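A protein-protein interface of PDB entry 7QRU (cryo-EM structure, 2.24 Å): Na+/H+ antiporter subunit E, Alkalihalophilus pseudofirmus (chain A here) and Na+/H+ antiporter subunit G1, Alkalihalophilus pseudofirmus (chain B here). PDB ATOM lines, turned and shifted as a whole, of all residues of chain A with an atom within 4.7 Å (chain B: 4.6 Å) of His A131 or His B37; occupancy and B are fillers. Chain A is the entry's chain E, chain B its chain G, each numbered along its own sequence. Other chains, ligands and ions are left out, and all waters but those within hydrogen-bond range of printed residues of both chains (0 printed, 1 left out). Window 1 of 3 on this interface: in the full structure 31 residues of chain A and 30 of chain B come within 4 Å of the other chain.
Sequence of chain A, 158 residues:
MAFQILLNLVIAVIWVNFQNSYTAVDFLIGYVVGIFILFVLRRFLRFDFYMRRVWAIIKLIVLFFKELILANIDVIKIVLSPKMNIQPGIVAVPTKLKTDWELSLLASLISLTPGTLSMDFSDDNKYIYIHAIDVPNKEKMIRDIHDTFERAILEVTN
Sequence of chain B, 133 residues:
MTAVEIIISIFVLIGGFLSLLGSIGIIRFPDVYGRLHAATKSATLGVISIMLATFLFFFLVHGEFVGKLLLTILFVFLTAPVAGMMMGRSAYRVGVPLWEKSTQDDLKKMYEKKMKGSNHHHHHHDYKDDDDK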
ATOM      1  N   PRO A  88      29.933  -1.020   5.650  1.00  0.00           N
ATOM      2  CA  PRO A  88      30.435  -1.245   7.015  1.00  0.00           C
ATOM      3  C   PRO A  88      31.870  -1.792   7.076  1.00  0.00           C
ATOM      4  O   PRO A  88      32.390  -2.203   6.061  1.00  0.00           O
ATOM      5  CB  PRO A  88      29.373  -2.198   7.603  1.00  0.00           C
ATOM      6  CG  PRO A  88      28.837  -2.890   6.429  1.00  0.00           C
ATOM      7  CD  PRO A  88      28.953  -1.997   5.225  1.00  0.00           C
ATOM      8  N   GLY A  89      32.464  -1.845   8.267  1.00  0.00           N
ATOM      9  CA  GLY A  89      33.770  -2.431   8.525  1.00  0.00           C
ATOM     10  C   GLY A  89      34.226  -2.241   9.973  1.00  0.00           C
ATOM     11  O   GLY A  89      33.539  -1.575  10.727  1.00  0.00           O
ATOM     12  N   ILE A  90      35.299  -2.952  10.371  1.00  0.00           N
ATOM     13  CA  ILE A  90      35.901  -2.846  11.693  1.00  0.00           C
ATOM     14  C   ILE A  90      37.190  -2.049  11.654  1.00  0.00           C
ATOM     15  O   ILE A  90      38.066  -2.420  10.954  1.00  0.00           O
ATOM     16  CB  ILE A  90      36.119  -4.198  12.377  1.00  0.00           C
ATOM     17  CG1 ILE A  90      34.816  -4.985  12.390  1.00  0.00           C
ATOM     18  CG2 ILE A  90      36.659  -3.997  13.809  1.00  0.00           C
ATOM     19  CD1 ILE A  90      34.707  -6.166  13.228  1.00  0.00           C
ATOM     20  N   GLY A 115      26.905   5.926  14.145  1.00  0.00           N
ATOM     21  CA  GLY A 115      27.533   5.053  13.163  1.00  0.00           C
ATOM     22  C   GLY A 115      28.436   4.000  13.747  1.00  0.00           C
ATOM     23  O   GLY A 115      29.021   3.243  12.982  1.00  0.00           O
ATOM     24  N   THR A 116      28.597   3.970  15.063  1.00  0.00           N
ATOM     25  CA  THR A 116      29.675   3.168  15.604  1.00  0.00           C
ATOM     26  C   THR A 116      29.242   2.245  16.722  1.00  0.00           C
ATOM     27  O   THR A 116      28.406   2.584  17.564  1.00  0.00           O
ATOM     28  CB  THR A 116      30.789   4.144  16.024  1.00  0.00           C
ATOM     29  OG1 THR A 116      30.283   5.175  16.885  1.00  0.00           O
ATOM     30  CG2 THR A 116      31.391   4.763  14.763  1.00  0.00           C
ATOM     31  N   LEU A 117      30.032   1.219  16.898  1.00  0.00           N
ATOM     32  CA  LEU A 117      29.826   0.306  17.986  1.00  0.00           C
ATOM     33  C   LEU A 117      31.141  -0.311  18.427  1.00  0.00           C
ATOM     34  O   LEU A 117      31.778  -0.900  17.596  1.00  0.00           O
ATOM     35  CB  LEU A 117      28.945  -0.747  17.376  1.00  0.00           C
ATOM     36  CG  LEU A 117      28.221  -1.615  18.353  1.00  0.00           C
ATOM     37  CD1 LEU A 117      26.952  -0.892  18.776  1.00  0.00           C
ATOM     38  CD2 LEU A 117      27.950  -2.926  17.659  1.00  0.00           C
ATOM     39  N   MET A 119      33.510  -2.910  19.564  1.00  0.00           N
ATOM     40  CA  MET A 119      33.593  -4.375  19.500  1.00  0.00           C
ATOM     41  C   MET A 119      34.505  -4.965  20.600  1.00  0.00           C
ATOM     42  O   MET A 119      34.163  -5.888  21.286  1.00  0.00           O
ATOM     43  CB  MET A 119      34.186  -4.786  18.156  1.00  0.00           C
ATOM     44  CG  MET A 119      33.337  -4.467  16.967  1.00  0.00           C
ATOM     45  SD  MET A 119      32.374  -5.899  16.554  1.00  0.00           S
ATOM     46  CE  MET A 119      30.941  -5.543  17.576  1.00  0.00           C
ATOM     47  N   TYR A 129      38.583  -1.444  19.009  1.00  0.00           N
ATOM     48  CA  TYR A 129      38.048  -1.937  17.707  1.00  0.00           C
ATOM     49  C   TYR A 129      36.605  -1.487  17.497  1.00  0.00           C
ATOM     50  O   TYR A 129      35.817  -1.651  18.406  1.00  0.00           O
ATOM     51  CB  TYR A 129      38.202  -3.454  17.542  1.00  0.00           C
ATOM     52  CG  TYR A 129      39.663  -3.808  17.392  1.00  0.00           C
ATOM     53  CD1 TYR A 129      40.292  -3.879  16.162  1.00  0.00           C
ATOM     54  CD2 TYR A 129      40.455  -3.874  18.529  1.00  0.00           C
ATOM     55  CE1 TYR A 129      41.652  -4.099  16.111  1.00  0.00           C
ATOM     56  CE2 TYR A 129      41.813  -4.048  18.484  1.00  0.00           C
ATOM     57  CZ  TYR A 129      42.410  -4.206  17.270  1.00  0.00           C
ATOM     58  OH  TYR A 129      43.762  -4.448  17.278  1.00  0.00           O
ATOM     59  N   ILE A 130      36.335  -0.739  16.418  1.00  0.00           N
ATOM     60  CA  ILE A 130      35.013  -0.172  16.218  1.00  0.00           C
ATOM     61  C   ILE A 130      34.284  -0.664  14.957  1.00  0.00           C
ATOM     62  O   ILE A 130      34.794  -0.526  13.868  1.00  0.00           O
ATOM     63  CB  ILE A 130      35.184   1.333  16.286  1.00  0.00           C
ATOM     64  CG1 ILE A 130      35.688   1.726  17.667  1.00  0.00           C
ATOM     65  CG2 ILE A 130      33.891   2.039  15.966  1.00  0.00           C
ATOM     66  CD1 ILE A 130      36.003   3.229  17.666  1.00  0.00           C
ATOM     67  N   HIS A 131      33.081  -1.239  15.143  1.00  0.00           N
ATOM     68  CA  HIS A 131      32.267  -1.597  14.020  1.00  0.00           C
ATOM     69  C   HIS A 131      31.582  -0.312  13.596  1.00  0.00           C
ATOM     70  O   HIS A 131      30.887   0.252  14.410  1.00  0.00           O
ATOM     71  CB  HIS A 131      31.240  -2.664  14.292  1.00  0.00           C
ATOM     72  CG  HIS A 131      30.525  -3.075  13.061  1.00  0.00           C
ATOM     73  ND1 HIS A 131      29.285  -2.569  12.679  1.00  0.00           N
ATOM     74  CD2 HIS A 131      30.892  -3.969  12.131  1.00  0.00           C
ATOM     75  CE1 HIS A 131      28.993  -3.032  11.476  1.00  0.00           C
ATOM     76  NE2 HIS A 131      29.920  -3.945  11.158  1.00  0.00           N
ATOM     77  N   ALA A 132      31.869   0.129  12.364  1.00  0.00           N
ATOM     78  CA  ALA A 132      31.377   1.343  11.772  1.00  0.00           C
ATOM     79  C   ALA A 132      30.462   0.992  10.631  1.00  0.00           C
ATOM     80  O   ALA A 132      30.684   0.007  10.012  1.00  0.00           O
ATOM     81  CB  ALA A 132      32.527   2.133  11.215  1.00  0.00           C
ATOM     82  N   ILE A 133      29.414   1.756  10.438  1.00  0.00           N
ATOM     83  CA  ILE A 133      28.371   1.470   9.447  1.00  0.00           C
ATOM     84  C   ILE A 133      28.788   2.103   8.112  1.00  0.00           C
ATOM     85  O   ILE A 133      28.398   1.604   7.081  1.00  0.00           O
ATOM     86  CB  ILE A 133      26.969   1.954   9.948  1.00  0.00           C
ATOM     87  CG1 ILE A 133      25.892   0.971   9.626  1.00  0.00           C
ATOM     88  CG2 ILE A 133      26.603   3.314   9.412  1.00  0.00           C
ATOM     89  CD1 ILE A 133      26.121  -0.340  10.319  1.00  0.00           C
ATOM     90  N   TYR B  33      26.140  -7.548  13.112  1.00  0.00           N
ATOM     91  CA  TYR B  33      26.869  -6.357  13.589  1.00  0.00           C
ATOM     92  C   TYR B  33      26.071  -5.070  13.359  1.00  0.00           C
ATOM     93  O   TYR B  33      25.999  -4.286  14.273  1.00  0.00           O
ATOM     94  CB  TYR B  33      28.209  -6.238  12.895  1.00  0.00           C
ATOM     95  CG  TYR B  33      28.971  -7.523  13.068  1.00  0.00           C
ATOM     96  CD1 TYR B  33      29.485  -7.855  14.309  1.00  0.00           C
ATOM     97  CD2 TYR B  33      29.099  -8.442  12.019  1.00  0.00           C
ATOM     98  CE1 TYR B  33      30.011  -9.112  14.560  1.00  0.00           C
ATOM     99  CE2 TYR B  33      29.625  -9.688  12.268  1.00  0.00           C
ATOM    100  CZ  TYR B  33      30.204  -9.966  13.499  1.00  0.00           C
ATOM    101  OH  TYR B  33      30.730 -11.220  13.650  1.00  0.00           O
ATOM    102  N   GLY B  34      25.401  -4.888  12.200  1.00  0.00           N
ATOM    103  CA  GLY B  34      24.566  -3.745  11.916  1.00  0.00           C
ATOM    104  C   GLY B  34      23.293  -3.847  12.754  1.00  0.00           C
ATOM    105  O   GLY B  34      22.707  -2.851  13.146  1.00  0.00           O
ATOM    106  N   ARG B  35      22.808  -5.037  12.986  1.00  0.00           N
ATOM    107  CA  ARG B  35      21.590  -5.173  13.782  1.00  0.00           C
ATOM    108  C   ARG B  35      21.873  -4.767  15.227  1.00  0.00           C
ATOM    109  O   ARG B  35      20.973  -4.381  15.923  1.00  0.00           O
ATOM    110  CB  ARG B  35      21.158  -6.637  13.721  1.00  0.00           C
ATOM    111  CG  ARG B  35      20.620  -7.026  12.355  1.00  0.00           C
ATOM    112  CD  ARG B  35      20.352  -8.523  12.365  1.00  0.00           C
ATOM    113  NE  ARG B  35      20.107  -8.781  10.974  1.00  0.00           N
ATOM    114  CZ  ARG B  35      20.589  -9.797  10.325  1.00  0.00           C
ATOM    115  NH1 ARG B  35      21.161 -10.756  11.022  1.00  0.00           N
ATOM    116  NH2 ARG B  35      20.421  -9.841   9.019  1.00  0.00           N
ATOM    117  N   LEU B  36      23.109  -4.924  15.733  1.00  0.00           N
ATOM    118  CA  LEU B  36      23.495  -4.426  17.042  1.00  0.00           C
ATOM    119  C   LEU B  36      23.456  -2.897  16.996  1.00  0.00           C
ATOM    120  O   LEU B  36      23.256  -2.281  18.027  1.00  0.00           O
ATOM    121  CB  LEU B  36      24.874  -4.970  17.497  1.00  0.00           C
ATOM    122  CG  LEU B  36      24.813  -6.353  18.055  1.00  0.00           C
ATOM    123  CD1 LEU B  36      26.151  -6.955  18.059  1.00  0.00           C
ATOM    124  CD2 LEU B  36      24.214  -6.352  19.418  1.00  0.00           C
ATOM    125  N   HIS B  37      23.679  -2.247  15.873  1.00  0.00           N
ATOM    126  CA  HIS B  37      23.512  -0.785  15.909  1.00  0.00           C
ATOM    127  C   HIS B  37      22.121  -0.365  16.306  1.00  0.00           C
ATOM    128  O   HIS B  37      21.990   0.479  17.173  1.00  0.00           O
ATOM    129  CB  HIS B  37      23.870  -0.120  14.607  1.00  0.00           C
ATOM    130  CG  HIS B  37      25.354  -0.154  14.411  1.00  0.00           C
ATOM    131  ND1 HIS B  37      26.136   0.982  14.308  1.00  0.00           N
ATOM    132  CD2 HIS B  37      26.195  -1.219  14.248  1.00  0.00           C
ATOM    133  CE1 HIS B  37      27.384   0.601  14.011  1.00  0.00           C
ATOM    134  NE2 HIS B  37      27.459  -0.757  13.959  1.00  0.00           N
ATOM    135  N   ALA B  38      21.089  -0.945  15.696  1.00  0.00           N
ATOM    136  CA  ALA B  38      19.704  -0.716  16.027  1.00  0.00           C
ATOM    137  C   ALA B  38      19.320  -1.152  17.441  1.00  0.00           C
ATOM    138  O   ALA B  38      18.542  -0.476  18.085  1.00  0.00           O
ATOM    139  CB  ALA B  38      18.895  -1.481  15.075  1.00  0.00           C
ATOM    140  N   ALA B  39      19.789  -2.295  17.878  1.00  0.00           N
ATOM    141  CA  ALA B  39      19.463  -2.799  19.181  1.00  0.00           C
ATOM    142  C   ALA B  39      20.043  -1.898  20.274  1.00  0.00           C
ATOM    143  O   ALA B  39      19.321  -1.333  21.068  1.00  0.00           O
ATOM    144  CB  ALA B  39      19.967  -4.201  19.320  1.00  0.00           C
ATOM    145  N   THR B  40      21.319  -1.642  20.224  1.00  0.00           N
ATOM    146  CA  THR B  40      22.004  -0.759  21.143  1.00  0.00           C
ATOM    147  C   THR B  40      21.547   0.702  21.103  1.00  0.00           C
ATOM    148  O   THR B  40      21.606   1.335  22.144  1.00  0.00           O
ATOM    149  CB  THR B  40      23.489  -0.912  20.881  1.00  0.00           C
ATOM    150  OG1 THR B  40      23.600  -2.353  20.954  1.00  0.00           O
ATOM    151  CG2 THR B  40      24.368  -0.237  21.906  1.00  0.00           C
ATOM    152  N   LYS B  41      21.164   1.279  19.973  1.00  0.00           N
ATOM    153  CA  LYS B  41      20.885   2.716  19.959  1.00  0.00           C
ATOM    154  C   LYS B  41      19.380   3.004  20.026  1.00  0.00           C
ATOM    155  O   LYS B  41      18.967   3.810  20.823  1.00  0.00           O
ATOM    156  CB  LYS B  41      21.450   3.390  18.725  1.00  0.00           C
ATOM    157  CG  LYS B  41      22.957   3.330  18.836  1.00  0.00           C
ATOM    158  CD  LYS B  41      23.708   3.463  17.525  1.00  0.00           C
ATOM    159  CE  LYS B  41      25.175   3.299  17.852  1.00  0.00           C
ATOM    160  NZ  LYS B  41      25.813   3.408  16.564  1.00  0.00           N
ATOM    161  N   SER B  42      18.554   2.403  19.145  1.00  0.00           N
ATOM    162  CA  SER B  42      17.143   2.757  19.052  1.00  0.00           C
ATOM    163  C   SER B  42      16.358   2.166  20.206  1.00  0.00           C
ATOM    164  O   SER B  42      15.580   2.851  20.840  1.00  0.00           O
ATOM    165  CB  SER B  42      16.581   2.393  17.711  1.00  0.00           C
ATOM    166  OG  SER B  42      17.269   3.144  16.755  1.00  0.00           O
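NZ of Lys B41 sits at hydrogen-bond distance from O of Thr A116, at 2.9 Å.
A ring nitrogen (NE2) of His B37 is in hydrogen-bond range of a ring nitrogen (ND1) of His A131 (2.9 Å).
N of His A131 lies within hydrogen-bond range of O of Leu A117 (2.8 Å).
The side-chain amino group (NZ) of Lys B41 sits at hydrogen-bond distance from a ring nitrogen (ND1) of His B37 (3.3 Å).
The backbone carbonyl oxygen (O) of Leu B36 lies within hydrogen-bond range of the side-chain hydroxyl (OG1) of Thr B40.
N of Ile A133 lies within hydrogen-bond range of O of Gly A115, 3.0 Å away.
Gly A115 touches His B37.
N of Gly A115 touches NZ of Lys B41 (3.7 Å).
His B37 touches Thr A116 (CE1 to C, 3.7 Å).
CD2 of Leu A117 touches CB of Leu B36, at 3.7 Å.
Leu A117 touches His B37.
NE2 of His A131 touches CB of Tyr B33 (3.3 Å).
CD1 of Ile A133 touches NE2 of His B37, 3.9 Å away.
Of the printed residues of chain B, Gly A115 touches His B37 and Lys B41.
Of the printed residues of chain B, Thr A116 touches His B37 and Lys B41.
Of the printed residues of chain B, Leu A117 touches Leu B36 (3.7 Å) and His B37 (3.7 Å).
Of chain B, only Tyr B33 and His B37 come within 4 Å of His A131.
His B37 touches five residues of chain A.
The nearest residue of chain B that does not touch His A131 is Gly B34 (4.1 Å).
The nearest residue of chain A that does not touch His B37 is Ala A132 (4.6 Å).
The nearest printed residue of chain A that does not touch Leu B36 is Met A119 (5.0 Å).
Hydrophobic or aromatic side chains of chain A within 4 Å of the printed part of chain B: Leu A117, His A131 and Ile A133.
Among the printed residues, 9 pairs touch across the chains.
Among the printed residues, no Asp or Glu carboxylate lies within 4 Å of a Lys or Arg side-chain nitrogen of the other chain.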
